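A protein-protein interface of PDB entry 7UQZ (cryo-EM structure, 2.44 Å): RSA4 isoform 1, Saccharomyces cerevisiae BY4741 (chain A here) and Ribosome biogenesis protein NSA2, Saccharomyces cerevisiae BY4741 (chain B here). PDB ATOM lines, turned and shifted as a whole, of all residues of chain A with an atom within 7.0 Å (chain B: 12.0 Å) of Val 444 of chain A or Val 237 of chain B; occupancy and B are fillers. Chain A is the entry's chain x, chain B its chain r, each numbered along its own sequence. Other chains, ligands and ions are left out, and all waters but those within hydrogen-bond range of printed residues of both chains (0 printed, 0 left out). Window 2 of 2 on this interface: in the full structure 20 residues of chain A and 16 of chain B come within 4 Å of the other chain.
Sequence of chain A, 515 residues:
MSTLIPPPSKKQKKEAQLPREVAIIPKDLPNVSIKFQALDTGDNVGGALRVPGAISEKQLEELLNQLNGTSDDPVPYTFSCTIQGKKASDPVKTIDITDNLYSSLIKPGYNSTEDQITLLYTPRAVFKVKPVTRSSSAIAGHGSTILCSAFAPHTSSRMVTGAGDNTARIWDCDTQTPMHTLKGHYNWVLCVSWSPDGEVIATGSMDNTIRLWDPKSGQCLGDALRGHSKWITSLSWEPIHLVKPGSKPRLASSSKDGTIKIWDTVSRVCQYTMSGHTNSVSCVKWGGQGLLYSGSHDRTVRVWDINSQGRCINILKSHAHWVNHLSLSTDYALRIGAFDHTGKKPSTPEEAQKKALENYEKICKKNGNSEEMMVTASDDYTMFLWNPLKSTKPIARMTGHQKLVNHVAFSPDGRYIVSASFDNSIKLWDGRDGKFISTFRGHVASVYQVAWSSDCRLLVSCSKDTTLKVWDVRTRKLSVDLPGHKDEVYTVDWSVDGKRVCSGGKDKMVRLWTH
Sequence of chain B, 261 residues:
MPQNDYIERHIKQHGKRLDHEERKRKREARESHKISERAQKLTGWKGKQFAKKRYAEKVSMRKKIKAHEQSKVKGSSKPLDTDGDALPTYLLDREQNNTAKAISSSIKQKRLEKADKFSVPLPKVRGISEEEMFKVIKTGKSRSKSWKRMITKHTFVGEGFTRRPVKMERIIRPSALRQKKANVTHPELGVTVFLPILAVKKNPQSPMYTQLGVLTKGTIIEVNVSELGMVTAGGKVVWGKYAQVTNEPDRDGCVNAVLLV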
ATOM      1  N   ASN A 424      22.292  -5.470   7.864  1.00  0.00           N
ATOM      2  CA  ASN A 424      22.711  -4.292   8.628  1.00  0.00           C
ATOM      3  C   ASN A 424      22.509  -2.997   7.850  1.00  0.00           C
ATOM      4  O   ASN A 424      23.270  -2.042   8.014  1.00  0.00           O
ATOM      5  CB  ASN A 424      24.169  -4.407   9.084  1.00  0.00           C
ATOM      6  CG  ASN A 424      24.483  -5.751   9.697  1.00  0.00           C
ATOM      7  OD1 ASN A 424      23.620  -6.622   9.786  1.00  0.00           O
ATOM      8  ND2 ASN A 424      25.729  -5.934  10.110  1.00  0.00           N
ATOM      9  N   GLY A 442      25.266   2.246   8.997  1.00  0.00           N
ATOM     10  CA  GLY A 442      25.667   2.656  10.326  1.00  0.00           C
ATOM     11  C   GLY A 442      25.329   1.634  11.391  1.00  0.00           C
ATOM     12  O   GLY A 442      26.000   1.566  12.424  1.00  0.00           O
ATOM     13  N   HIS A 443      24.293   0.834  11.157  1.00  0.00           N
ATOM     14  CA  HIS A 443      24.014  -0.290  12.039  1.00  0.00           C
ATOM     15  C   HIS A 443      25.035  -1.397  11.811  1.00  0.00           C
ATOM     16  O   HIS A 443      25.368  -1.730  10.672  1.00  0.00           O
ATOM     17  CB  HIS A 443      22.601  -0.825  11.805  1.00  0.00           C
ATOM     18  CG  HIS A 443      21.520   0.034  12.380  1.00  0.00           C
ATOM     19  ND1 HIS A 443      21.483   0.395  13.709  1.00  0.00           N
ATOM     20  CD2 HIS A 443      20.428   0.594  11.809  1.00  0.00           C
ATOM     21  CE1 HIS A 443      20.418   1.142  13.931  1.00  0.00           C
ATOM     22  NE2 HIS A 443      19.761   1.279  12.794  1.00  0.00           N
ATOM     23  N   VAL A 444      25.543  -1.964  12.907  1.00  0.00           N
ATOM     24  CA  VAL A 444      26.510  -3.052  12.822  1.00  0.00           C
ATOM     25  C   VAL A 444      25.868  -4.412  13.038  1.00  0.00           C
ATOM     26  O   VAL A 444      26.573  -5.430  13.027  1.00  0.00           O
ATOM     27  CB  VAL A 444      27.673  -2.844  13.811  1.00  0.00           C
ATOM     28  CG1 VAL A 444      28.517  -1.659  13.382  1.00  0.00           C
ATOM     29  CG2 VAL A 444      27.148  -2.644  15.219  1.00  0.00           C
ATOM     30  N   ALA A 445      24.555  -4.461  13.238  1.00  0.00           N
ATOM     31  CA  ALA A 445      23.803  -5.702  13.325  1.00  0.00           C
ATOM     32  C   ALA A 445      22.533  -5.556  12.495  1.00  0.00           C
ATOM     33  O   ALA A 445      22.254  -4.493  11.933  1.00  0.00           O
ATOM     34  CB  ALA A 445      23.484  -6.061  14.780  1.00  0.00           C
ATOM     35  N   SER A 446      21.764  -6.639  12.414  1.00  0.00           N
ATOM     36  CA  SER A 446      20.588  -6.666  11.556  1.00  0.00           C
ATOM     37  C   SER A 446      19.529  -5.685  12.047  1.00  0.00           C
ATOM     38  O   SER A 446      19.244  -5.597  13.243  1.00  0.00           O
ATOM     39  CB  SER A 446      20.007  -8.078  11.496  1.00  0.00           C
ATOM     40  OG  SER A 446      19.501  -8.477  12.755  1.00  0.00           O
ATOM     41  N   VAL A 447      18.950  -4.943  11.109  1.00  0.00           N
ATOM     42  CA  VAL A 447      17.905  -3.978  11.430  1.00  0.00           C
ATOM     43  C   VAL A 447      16.575  -4.711  11.532  1.00  0.00           C
ATOM     44  O   VAL A 447      16.186  -5.448  10.620  1.00  0.00           O
ATOM     45  CB  VAL A 447      17.846  -2.866  10.373  1.00  0.00           C
ATOM     46  CG1 VAL A 447      17.021  -1.696  10.881  1.00  0.00           C
ATOM     47  CG2 VAL A 447      19.249  -2.417   9.994  1.00  0.00           C
ATOM     48  N   SER A 463      17.710  -1.631  15.977  1.00  0.00           N
ATOM     49  CA  SER A 463      18.535  -2.721  15.473  1.00  0.00           C
ATOM     50  C   SER A 463      18.902  -3.708  16.573  1.00  0.00           C
ATOM     51  O   SER A 463      18.701  -3.469  17.766  1.00  0.00           O
ATOM     52  CB  SER A 463      19.806  -2.190  14.801  1.00  0.00           C
ATOM     53  OG  SER A 463      20.664  -3.247  14.410  1.00  0.00           O
ATOM     54  N   LYS A 464      19.446  -4.842  16.124  1.00  0.00           N
ATOM     55  CA  LYS A 464      19.982  -5.875  17.001  1.00  0.00           C
ATOM     56  C   LYS A 464      21.224  -5.408  17.752  1.00  0.00           C
ATOM     57  O   LYS A 464      21.610  -6.037  18.742  1.00  0.00           O
ATOM     58  CB  LYS A 464      20.292  -7.121  16.164  1.00  0.00           C
ATOM     59  CG  LYS A 464      20.610  -8.392  16.926  1.00  0.00           C
ATOM     60  CD  LYS A 464      21.101  -9.475  15.979  1.00  0.00           C
ATOM     61  CE  LYS A 464      21.227 -10.819  16.676  1.00  0.00           C
ATOM     62  NZ  LYS A 464      22.172 -10.775  17.822  1.00  0.00           N
ATOM     63  N   ASP A 465      21.833  -4.299  17.331  1.00  0.00           N
ATOM     64  CA  ASP A 465      23.048  -3.808  17.968  1.00  0.00           C
ATOM     65  C   ASP A 465      22.722  -2.899  19.148  1.00  0.00           C
ATOM     66  O   ASP A 465      23.520  -2.026  19.502  1.00  0.00           O
ATOM     67  CB  ASP A 465      23.940  -3.081  16.953  1.00  0.00           C
ATOM     68  CG  ASP A 465      23.210  -1.983  16.185  1.00  0.00           C
ATOM     69  OD1 ASP A 465      22.217  -1.423  16.691  1.00  0.00           O
ATOM     70  OD2 ASP A 465      23.642  -1.676  15.057  1.00  0.00           O
ATOM     71  N   THR A 467      20.775  -0.433  19.527  1.00  0.00           N
ATOM     72  CA  THR A 467      20.742   0.997  19.262  1.00  0.00           C
ATOM     73  C   THR A 467      19.585   1.362  18.342  1.00  0.00           C
ATOM     74  O   THR A 467      19.102   0.546  17.541  1.00  0.00           O
ATOM     75  CB  THR A 467      22.051   1.502  18.627  1.00  0.00           C
ATOM     76  OG1 THR A 467      22.342   0.739  17.451  1.00  0.00           O
ATOM     77  CG2 THR A 467      23.213   1.399  19.605  1.00  0.00           C
ATOM     78  N   LYS A 469      18.577   4.568  15.514  1.00  0.00           N
ATOM     79  CA  LYS A 469      19.221   5.578  14.686  1.00  0.00           C
ATOM     80  C   LYS A 469      18.164   6.432  14.009  1.00  0.00           C
ATOM     81  O   LYS A 469      17.186   5.902  13.471  1.00  0.00           O
ATOM     82  CB  LYS A 469      20.152   4.945  13.644  1.00  0.00           C
ATOM     83  CG  LYS A 469      21.485   4.500  14.224  1.00  0.00           C
ATOM     84  CD  LYS A 469      22.457   4.037  13.161  1.00  0.00           C
ATOM     85  CE  LYS A 469      23.797   3.683  13.780  1.00  0.00           C
ATOM     86  NZ  LYS A 469      23.658   2.672  14.862  1.00  0.00           N
ATOM     87  N   ASP A 481      22.671   8.996  16.475  1.00  0.00           N
ATOM     88  CA  ASP A 481      22.727   7.632  16.982  1.00  0.00           C
ATOM     89  C   ASP A 481      22.312   7.628  18.448  1.00  0.00           C
ATOM     90  O   ASP A 481      22.794   8.450  19.234  1.00  0.00           O
ATOM     91  CB  ASP A 481      24.141   7.066  16.828  1.00  0.00           C
ATOM     92  CG  ASP A 481      24.286   5.677  17.417  1.00  0.00           C
ATOM     93  OD1 ASP A 481      23.288   4.928  17.456  1.00  0.00           O
ATOM     94  OD2 ASP A 481      25.408   5.336  17.851  1.00  0.00           O
ATOM     95  N   LEU B 189      25.342 -16.439  23.273  1.00  0.00           N
ATOM     96  CA  LEU B 189      24.734 -16.740  21.975  1.00  0.00           C
ATOM     97  C   LEU B 189      25.334 -17.983  21.324  1.00  0.00           C
ATOM     98  O   LEU B 189      24.819 -18.453  20.305  1.00  0.00           O
ATOM     99  CB  LEU B 189      24.831 -15.546  21.016  1.00  0.00           C
ATOM    100  CG  LEU B 189      24.204 -14.224  21.465  1.00  0.00           C
ATOM    101  CD1 LEU B 189      24.466 -13.136  20.432  1.00  0.00           C
ATOM    102  CD2 LEU B 189      22.714 -14.389  21.709  1.00  0.00           C
ATOM    103  N   VAL B 193      32.972 -17.926  15.177  1.00  0.00           N
ATOM    104  CA  VAL B 193      33.215 -17.134  13.978  1.00  0.00           C
ATOM    105  C   VAL B 193      34.696 -17.198  13.629  1.00  0.00           C
ATOM    106  O   VAL B 193      35.559 -17.264  14.509  1.00  0.00           O
ATOM    107  CB  VAL B 193      32.764 -15.660  14.147  1.00  0.00           C
ATOM    108  CG1 VAL B 193      32.585 -14.994  12.792  1.00  0.00           C
ATOM    109  CG2 VAL B 193      31.480 -15.565  14.953  1.00  0.00           C
ATOM    110  N   LEU B 195      37.681 -15.286  12.735  1.00  0.00           N
ATOM    111  CA  LEU B 195      38.072 -13.895  12.914  1.00  0.00           C
ATOM    112  C   LEU B 195      39.560 -13.701  12.650  1.00  0.00           C
ATOM    113  O   LEU B 195      40.365 -14.581  12.969  1.00  0.00           O
ATOM    114  CB  LEU B 195      37.754 -13.416  14.338  1.00  0.00           C
ATOM    115  CG  LEU B 195      36.307 -13.536  14.812  1.00  0.00           C
ATOM    116  CD1 LEU B 195      36.160 -13.004  16.226  1.00  0.00           C
ATOM    117  CD2 LEU B 195      35.386 -12.803  13.863  1.00  0.00           C
ATOM    118  N   LEU B 198      44.701  -9.878  15.434  1.00  0.00           N
ATOM    119  CA  LEU B 198      45.274  -8.537  15.455  1.00  0.00           C
ATOM    120  C   LEU B 198      46.636  -8.476  16.131  1.00  0.00           C
ATOM    121  O   LEU B 198      47.548  -7.825  15.614  1.00  0.00           O
ATOM    122  CB  LEU B 198      44.317  -7.563  16.149  1.00  0.00           C
ATOM    123  CG  LEU B 198      43.019  -7.247  15.405  1.00  0.00           C
ATOM    124  CD1 LEU B 198      42.093  -6.403  16.263  1.00  0.00           C
ATOM    125  CD2 LEU B 198      43.325  -6.540  14.095  1.00  0.00           C
ATOM    126  N   GLU B 222      44.643 -10.798  20.462  1.00  0.00           N
ATOM    127  CA  GLU B 222      43.675  -9.766  20.121  1.00  0.00           C
ATOM    128  C   GLU B 222      43.052 -10.101  18.773  1.00  0.00           C
ATOM    129  O   GLU B 222      43.766 -10.395  17.809  1.00  0.00           O
ATOM    130  CB  GLU B 222      44.331  -8.383  20.075  1.00  0.00           C
ATOM    131  CG  GLU B 222      43.354  -7.244  19.836  1.00  0.00           C
ATOM    132  CD  GLU B 222      44.048  -5.908  19.656  1.00  0.00           C
ATOM    133  OE1 GLU B 222      45.295  -5.884  19.609  1.00  0.00           O
ATOM    134  OE2 GLU B 222      43.346  -4.882  19.562  1.00  0.00           O
ATOM    135  N   VAL B 223      41.726 -10.058  18.711  1.00  0.00           N
ATOM    136  CA  VAL B 223      40.986 -10.467  17.526  1.00  0.00           C
ATOM    137  C   VAL B 223      40.040  -9.354  17.102  1.00  0.00           C
ATOM    138  O   VAL B 223      39.597  -8.533  17.914  1.00  0.00           O
ATOM    139  CB  VAL B 223      40.204 -11.781  17.758  1.00  0.00           C
ATOM    140  CG1 VAL B 223      41.163 -12.949  17.906  1.00  0.00           C
ATOM    141  CG2 VAL B 223      39.315 -11.666  18.983  1.00  0.00           C
ATOM    142  N   ASN B 224      39.736  -9.341  15.807  1.00  0.00           N
ATOM    143  CA  ASN B 224      38.797  -8.396  15.218  1.00  0.00           C
ATOM    144  C   ASN B 224      37.380  -8.930  15.393  1.00  0.00           C
ATOM    145  O   ASN B 224      37.067 -10.035  14.938  1.00  0.00           O
ATOM    146  CB  ASN B 224      39.133  -8.194  13.742  1.00  0.00           C
ATOM    147  CG  ASN B 224      38.439  -6.993  13.131  1.00  0.00           C
ATOM    148  OD1 ASN B 224      37.382  -6.562  13.585  1.00  0.00           O
ATOM    149  ND2 ASN B 224      39.036  -6.451  12.079  1.00  0.00           N
ATOM    150  N   VAL B 225      36.525  -8.146  16.046  1.00  0.00           N
ATOM    151  CA  VAL B 225      35.169  -8.576  16.372  1.00  0.00           C
ATOM    152  C   VAL B 225      34.153  -7.681  15.676  1.00  0.00           C
ATOM    153  O   VAL B 225      33.058  -7.447  16.201  1.00  0.00           O
ATOM    154  CB  VAL B 225      34.944  -8.584  17.896  1.00  0.00           C
ATOM    155  CG1 VAL B 225      35.733  -9.710  18.539  1.00  0.00           C
ATOM    156  CG2 VAL B 225      35.335  -7.245  18.502  1.00  0.00           C
ATOM    157  N   SER B 226      34.509  -7.177  14.491  1.00  0.00           N
ATOM    158  CA  SER B 226      33.637  -6.245  13.781  1.00  0.00           C
ATOM    159  C   SER B 226      32.317  -6.895  13.388  1.00  0.00           C
ATOM    160  O   SER B 226      31.256  -6.268  13.482  1.00  0.00           O
ATOM    161  CB  SER B 226      34.346  -5.706  12.540  1.00  0.00           C
ATOM    162  OG  SER B 226      35.619  -5.179  12.860  1.00  0.00           O
ATOM    163  N   GLU B 227      32.359  -8.151  12.942  1.00  0.00           N
ATOM    164  CA  GLU B 227      31.148  -8.813  12.476  1.00  0.00           C
ATOM    165  C   GLU B 227      30.218  -9.225  13.611  1.00  0.00           C
ATOM    166  O   GLU B 227      29.069  -9.590  13.340  1.00  0.00           O
ATOM    167  CB  GLU B 227      31.506 -10.036  11.626  1.00  0.00           C
ATOM    168  CG  GLU B 227      32.635 -10.896  12.173  1.00  0.00           C
ATOM    169  CD  GLU B 227      34.003 -10.472  11.657  1.00  0.00           C
ATOM    170  OE1 GLU B 227      34.544  -9.462  12.156  1.00  0.00           O
ATOM    171  OE2 GLU B 227      34.534 -11.151  10.752  1.00  0.00           O
ATOM    172  N   LEU B 228      30.672  -9.166  14.861  1.00  0.00           N
ATOM    173  CA  LEU B 228      29.821  -9.505  15.994  1.00  0.00           C
ATOM    174  C   LEU B 228      28.869  -8.383  16.384  1.00  0.00           C
ATOM    175  O   LEU B 228      27.911  -8.640  17.119  1.00  0.00           O
ATOM    176  CB  LEU B 228      30.681  -9.892  17.198  1.00  0.00           C
ATOM    177  CG  LEU B 228      31.483 -11.183  17.042  1.00  0.00           C
ATOM    178  CD1 LEU B 228      32.368 -11.418  18.252  1.00  0.00           C
ATOM    179  CD2 LEU B 228      30.547 -12.358  16.822  1.00  0.00           C
ATOM    180  N   GLY B 229      29.101  -7.160  15.910  1.00  0.00           N
ATOM    181  CA  GLY B 229      28.194  -6.057  16.155  1.00  0.00           C
ATOM    182  C   GLY B 229      28.057  -5.631  17.602  1.00  0.00           C
ATOM    183  O   GLY B 229      26.940  -5.440  18.091  1.00  0.00           O
ATOM    184  N   MET B 230      29.178  -5.480  18.301  1.00  0.00           N
ATOM    185  CA  MET B 230      29.170  -5.051  19.692  1.00  0.00           C
ATOM    186  C   MET B 230      29.266  -3.534  19.778  1.00  0.00           C
ATOM    187  O   MET B 230      30.123  -2.921  19.134  1.00  0.00           O
ATOM    188  CB  MET B 230      30.321  -5.688  20.465  1.00  0.00           C
ATOM    189  CG  MET B 230      30.250  -7.190  20.559  1.00  0.00           C
ATOM    190  SD  MET B 230      31.547  -7.827  21.627  1.00  0.00           S
ATOM    191  CE  MET B 230      31.351  -9.576  21.361  1.00  0.00           C
ATOM    192  N   VAL B 231      28.388  -2.937  20.580  1.00  0.00           N
ATOM    193  CA  VAL B 231      28.348  -1.497  20.800  1.00  0.00           C
ATOM    194  C   VAL B 231      28.444  -1.243  22.300  1.00  0.00           C
ATOM    195  O   VAL B 231      27.810  -1.942  23.097  1.00  0.00           O
ATOM    196  CB  VAL B 231      27.063  -0.869  20.213  1.00  0.00           C
ATOM    197  CG1 VAL B 231      27.041   0.631  20.432  1.00  0.00           C
ATOM    198  CG2 VAL B 231      26.944  -1.182  18.728  1.00  0.00           C
ATOM    199  N   THR B 232      29.244  -0.250  22.684  1.00  0.00           N
ATOM    200  CA  THR B 232      29.428   0.096  24.088  1.00  0.00           C
ATOM    201  C   THR B 232      28.212   0.863  24.607  1.00  0.00           C
ATOM    202  O   THR B 232      27.197   1.016  23.923  1.00  0.00           O
ATOM    203  CB  THR B 232      30.705   0.911  24.275  1.00  0.00           C
ATOM    204  OG1 THR B 232      30.596   2.142  23.551  1.00  0.00           O
ATOM    205  CG2 THR B 232      31.911   0.142  23.778  1.00  0.00           C
ATOM    206  N   ALA B 233      28.305   1.354  25.845  1.00  0.00           N
ATOM    207  CA  ALA B 233      27.251   2.204  26.386  1.00  0.00           C
ATOM    208  C   ALA B 233      27.242   3.575  25.725  1.00  0.00           C
ATOM    209  O   ALA B 233      26.180   4.193  25.596  1.00  0.00           O
ATOM    210  CB  ALA B 233      27.409   2.345  27.899  1.00  0.00           C
ATOM    211  N   GLY B 234      28.403   4.063  25.304  1.00  0.00           N
ATOM    212  CA  GLY B 234      28.543   5.358  24.677  1.00  0.00           C
ATOM    213  C   GLY B 234      28.315   5.387  23.183  1.00  0.00           C
ATOM    214  O   GLY B 234      28.506   6.438  22.563  1.00  0.00           O
ATOM    215  N   GLY B 235      27.911   4.273  22.581  1.00  0.00           N
ATOM    216  CA  GLY B 235      27.658   4.229  21.157  1.00  0.00           C
ATOM    217  C   GLY B 235      28.856   3.930  20.285  1.00  0.00           C
ATOM    218  O   GLY B 235      28.748   4.049  19.059  1.00  0.00           O
ATOM    219  N   LYS B 236      29.991   3.556  20.867  1.00  0.00           N
ATOM    220  CA  LYS B 236      31.159   3.193  20.078  1.00  0.00           C
ATOM    221  C   LYS B 236      31.063   1.744  19.619  1.00  0.00           C
ATOM    222  O   LYS B 236      30.658   0.860  20.379  1.00  0.00           O
ATOM    223  CB  LYS B 236      32.441   3.397  20.883  1.00  0.00           C
ATOM    224  CG  LYS B 236      33.115   4.744  20.672  1.00  0.00           C
ATOM    225  CD  LYS B 236      32.398   5.855  21.406  1.00  0.00           C
ATOM    226  CE  LYS B 236      33.215   7.135  21.385  1.00  0.00           C
ATOM    227  NZ  LYS B 236      32.599   8.192  22.230  1.00  0.00           N
ATOM    228  N   VAL B 237      31.444   1.504  18.369  1.00  0.00           N
ATOM    229  CA  VAL B 237      31.432   0.159  17.805  1.00  0.00           C
ATOM    230  C   VAL B 237      32.719  -0.549  18.205  1.00  0.00           C
ATOM    231  O   VAL B 237      33.819  -0.057  17.936  1.00  0.00           O
ATOM    232  CB  VAL B 237      31.277   0.203  16.279  1.00  0.00           C
ATOM    233  CG1 VAL B 237      31.413  -1.193  15.690  1.00  0.00           C
ATOM    234  CG2 VAL B 237      29.941   0.821  15.902  1.00  0.00           C
ATOM    235  N   VAL B 238      32.586  -1.708  18.841  1.00  0.00           N
ATOM    236  CA  VAL B 238      33.742  -2.507  19.226  1.00  0.00           C
ATOM    237  C   VAL B 238      34.191  -3.336  18.031  1.00  0.00           C
ATOM    238  O   VAL B 238      33.390  -4.057  17.425  1.00  0.00           O
ATOM    239  CB  VAL B 238      33.409  -3.411  20.425  1.00  0.00           C
ATOM    240  CG1 VAL B 238      34.672  -4.046  20.979  1.00  0.00           C
ATOM    241  CG2 VAL B 238      32.678  -2.631  21.500  1.00  0.00           C
ATOM    242  N   TRP B 239      35.474  -3.236  17.684  1.00  0.00           N
ATOM    243  CA  TRP B 239      36.030  -4.045  16.608  1.00  0.00           C
ATOM    244  C   TRP B 239      37.327  -4.741  17.009  1.00  0.00           C
ATOM    245  O   TRP B 239      37.957  -5.382  16.162  1.00  0.00           O
ATOM    246  CB  TRP B 239      36.244  -3.196  15.347  1.00  0.00           C
ATOM    247  CG  TRP B 239      37.361  -2.211  15.423  1.00  0.00           C
ATOM    248  CD1 TRP B 239      37.343  -0.992  16.034  1.00  0.00           C
ATOM    249  CD2 TRP B 239      38.661  -2.348  14.839  1.00  0.00           C
ATOM    250  NE1 TRP B 239      38.555  -0.368  15.877  1.00  0.00           N
ATOM    251  CE2 TRP B 239      39.381  -1.180  15.146  1.00  0.00           C
ATOM    252  CE3 TRP B 239      39.287  -3.349  14.089  1.00  0.00           C
ATOM    253  CZ2 TRP B 239      40.694  -0.985  14.731  1.00  0.00           C
ATOM    254  CZ3 TRP B 239      40.590  -3.153  13.679  1.00  0.00           C
ATOM    255  CH2 TRP B 239      41.279  -1.981  14.002  1.00  0.00           C
ATOM    256  N   GLY B 240      37.726  -4.654  18.273  1.00  0.00           N
ATOM    257  CA  GLY B 240      38.871  -5.398  18.761  1.00  0.00           C
ATOM    258  C   GLY B 240      38.683  -5.869  20.188  1.00  0.00           C
ATOM    259  O   GLY B 240      38.336  -5.070  21.061  1.00  0.00           O
ATOM    260  N   LYS B 241      38.906  -7.158  20.446  1.00  0.00           N
ATOM    261  CA  LYS B 241      38.760  -7.706  21.791  1.00  0.00           C
ATOM    262  C   LYS B 241      39.849  -8.740  22.039  1.00  0.00           C
ATOM    263  O   LYS B 241      40.688  -9.009  21.177  1.00  0.00           O
ATOM    264  CB  LYS B 241      37.369  -8.315  22.006  1.00  0.00           C
ATOM    265  CG  LYS B 241      36.289  -7.298  22.328  1.00  0.00           C
ATOM    266  CD  LYS B 241      34.980  -7.970  22.694  1.00  0.00           C
ATOM    267  CE  LYS B 241      35.109  -8.787  23.968  1.00  0.00           C
ATOM    268  NZ  LYS B 241      35.486  -7.951  25.139  1.00  0.00           N
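Along chain A the printed residues that touch a printed residue of chain B span positions 444 to 481.
Printed residues of chain B that touch a printed residue of chain A: Gly 229, Val 231, Gly 235 and Val 237.
Hydrophobic or aromatic side chains of chain B within 4 Å of the printed part of chain A: Val 231 and Val 237.
Among the printed residues, no Asp or Glu carboxylate lies within 4 Å of a Lys or Arg side-chain nitrogen of the other chain.
OD1 of Asp 465 of chain A sits close to OG of Ser 463 of chain A.
The backbone NH (N) of Ala 445 of chain A lies within hydrogen-bond range of the side-chain carboxylate (OD2) of Asp 465 of chain A.
O of Val 444 of chain A is in hydrogen-bond range of ND2 of Asn 424 of chain A (3.1 Å).
NZ of Lys 469 of chain A is in salt-bridge range of OD1 of Asp 481 of chain A (3.5 Å).
The side-chain carboxylate (OD2) of Asp 465 of chain A lies within hydrogen-bond range of the backbone NH (N) of Val 444 of chain A, 2.9 Å away.
A ring nitrogen (ND1) of His 443 of chain A is in hydrogen-bond range of the side-chain carboxylate of Asp 465 of chain A, 3.3 Å away.
Val 444 of chain A touches Gly 229 of chain B.
CG2 of Val 231 of chain B touches CG2 of Val 444 of chain A, at 3.8 Å.
Val 237 of chain B touches Val 444 of chain A (CG1 to CG1, 3.7 Å).
Gly 229 of chain B touches Asp 465 of chain A.
Asp 465 of chain A touches Val 231 of chain B.
CG2 of Thr 467 of chain A touches CG1 of Val 231 of chain B (3.99 Å).
Asp 481 of chain A touches Gly 235 of chain B.
No residue of chain B comes within 4 Å of Asn 424 of chain A.
No residue of chain B comes within 4 Å of His 443 of chain A.
Val 444 of chain A touches just these residues of chain B: Gly 229 (3.6 Å), Val 231 (3.8 Å) and Val 237 (3.7 Å).
No residue of chain B comes within 4 Å of Ala 445 of chain A.
Printed residues of chain B within 4 Å of Thr 467 of chain A: Val 231.
Printed residues of chain A within 4 Å of Gly 229 of chain B: Val 444 and Asp 465.
Printed residues of chain A within 4 Å of Val 231 of chain B: Val 444 (3.8 Å), Asp 465 (3.6 Å) and Thr 467 (3.99 Å).
Of chain A, only Val 444 comes within 4 Å of Val 237 of chain B.
The nearest residue of chain A that does not touch Val 237 of chain B is Gly 442 of chain A (5.3 Å).
The nearest printed residue of chain A that does not touch Val 231 of chain B is Asp 481 of chain A (5.6 Å).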
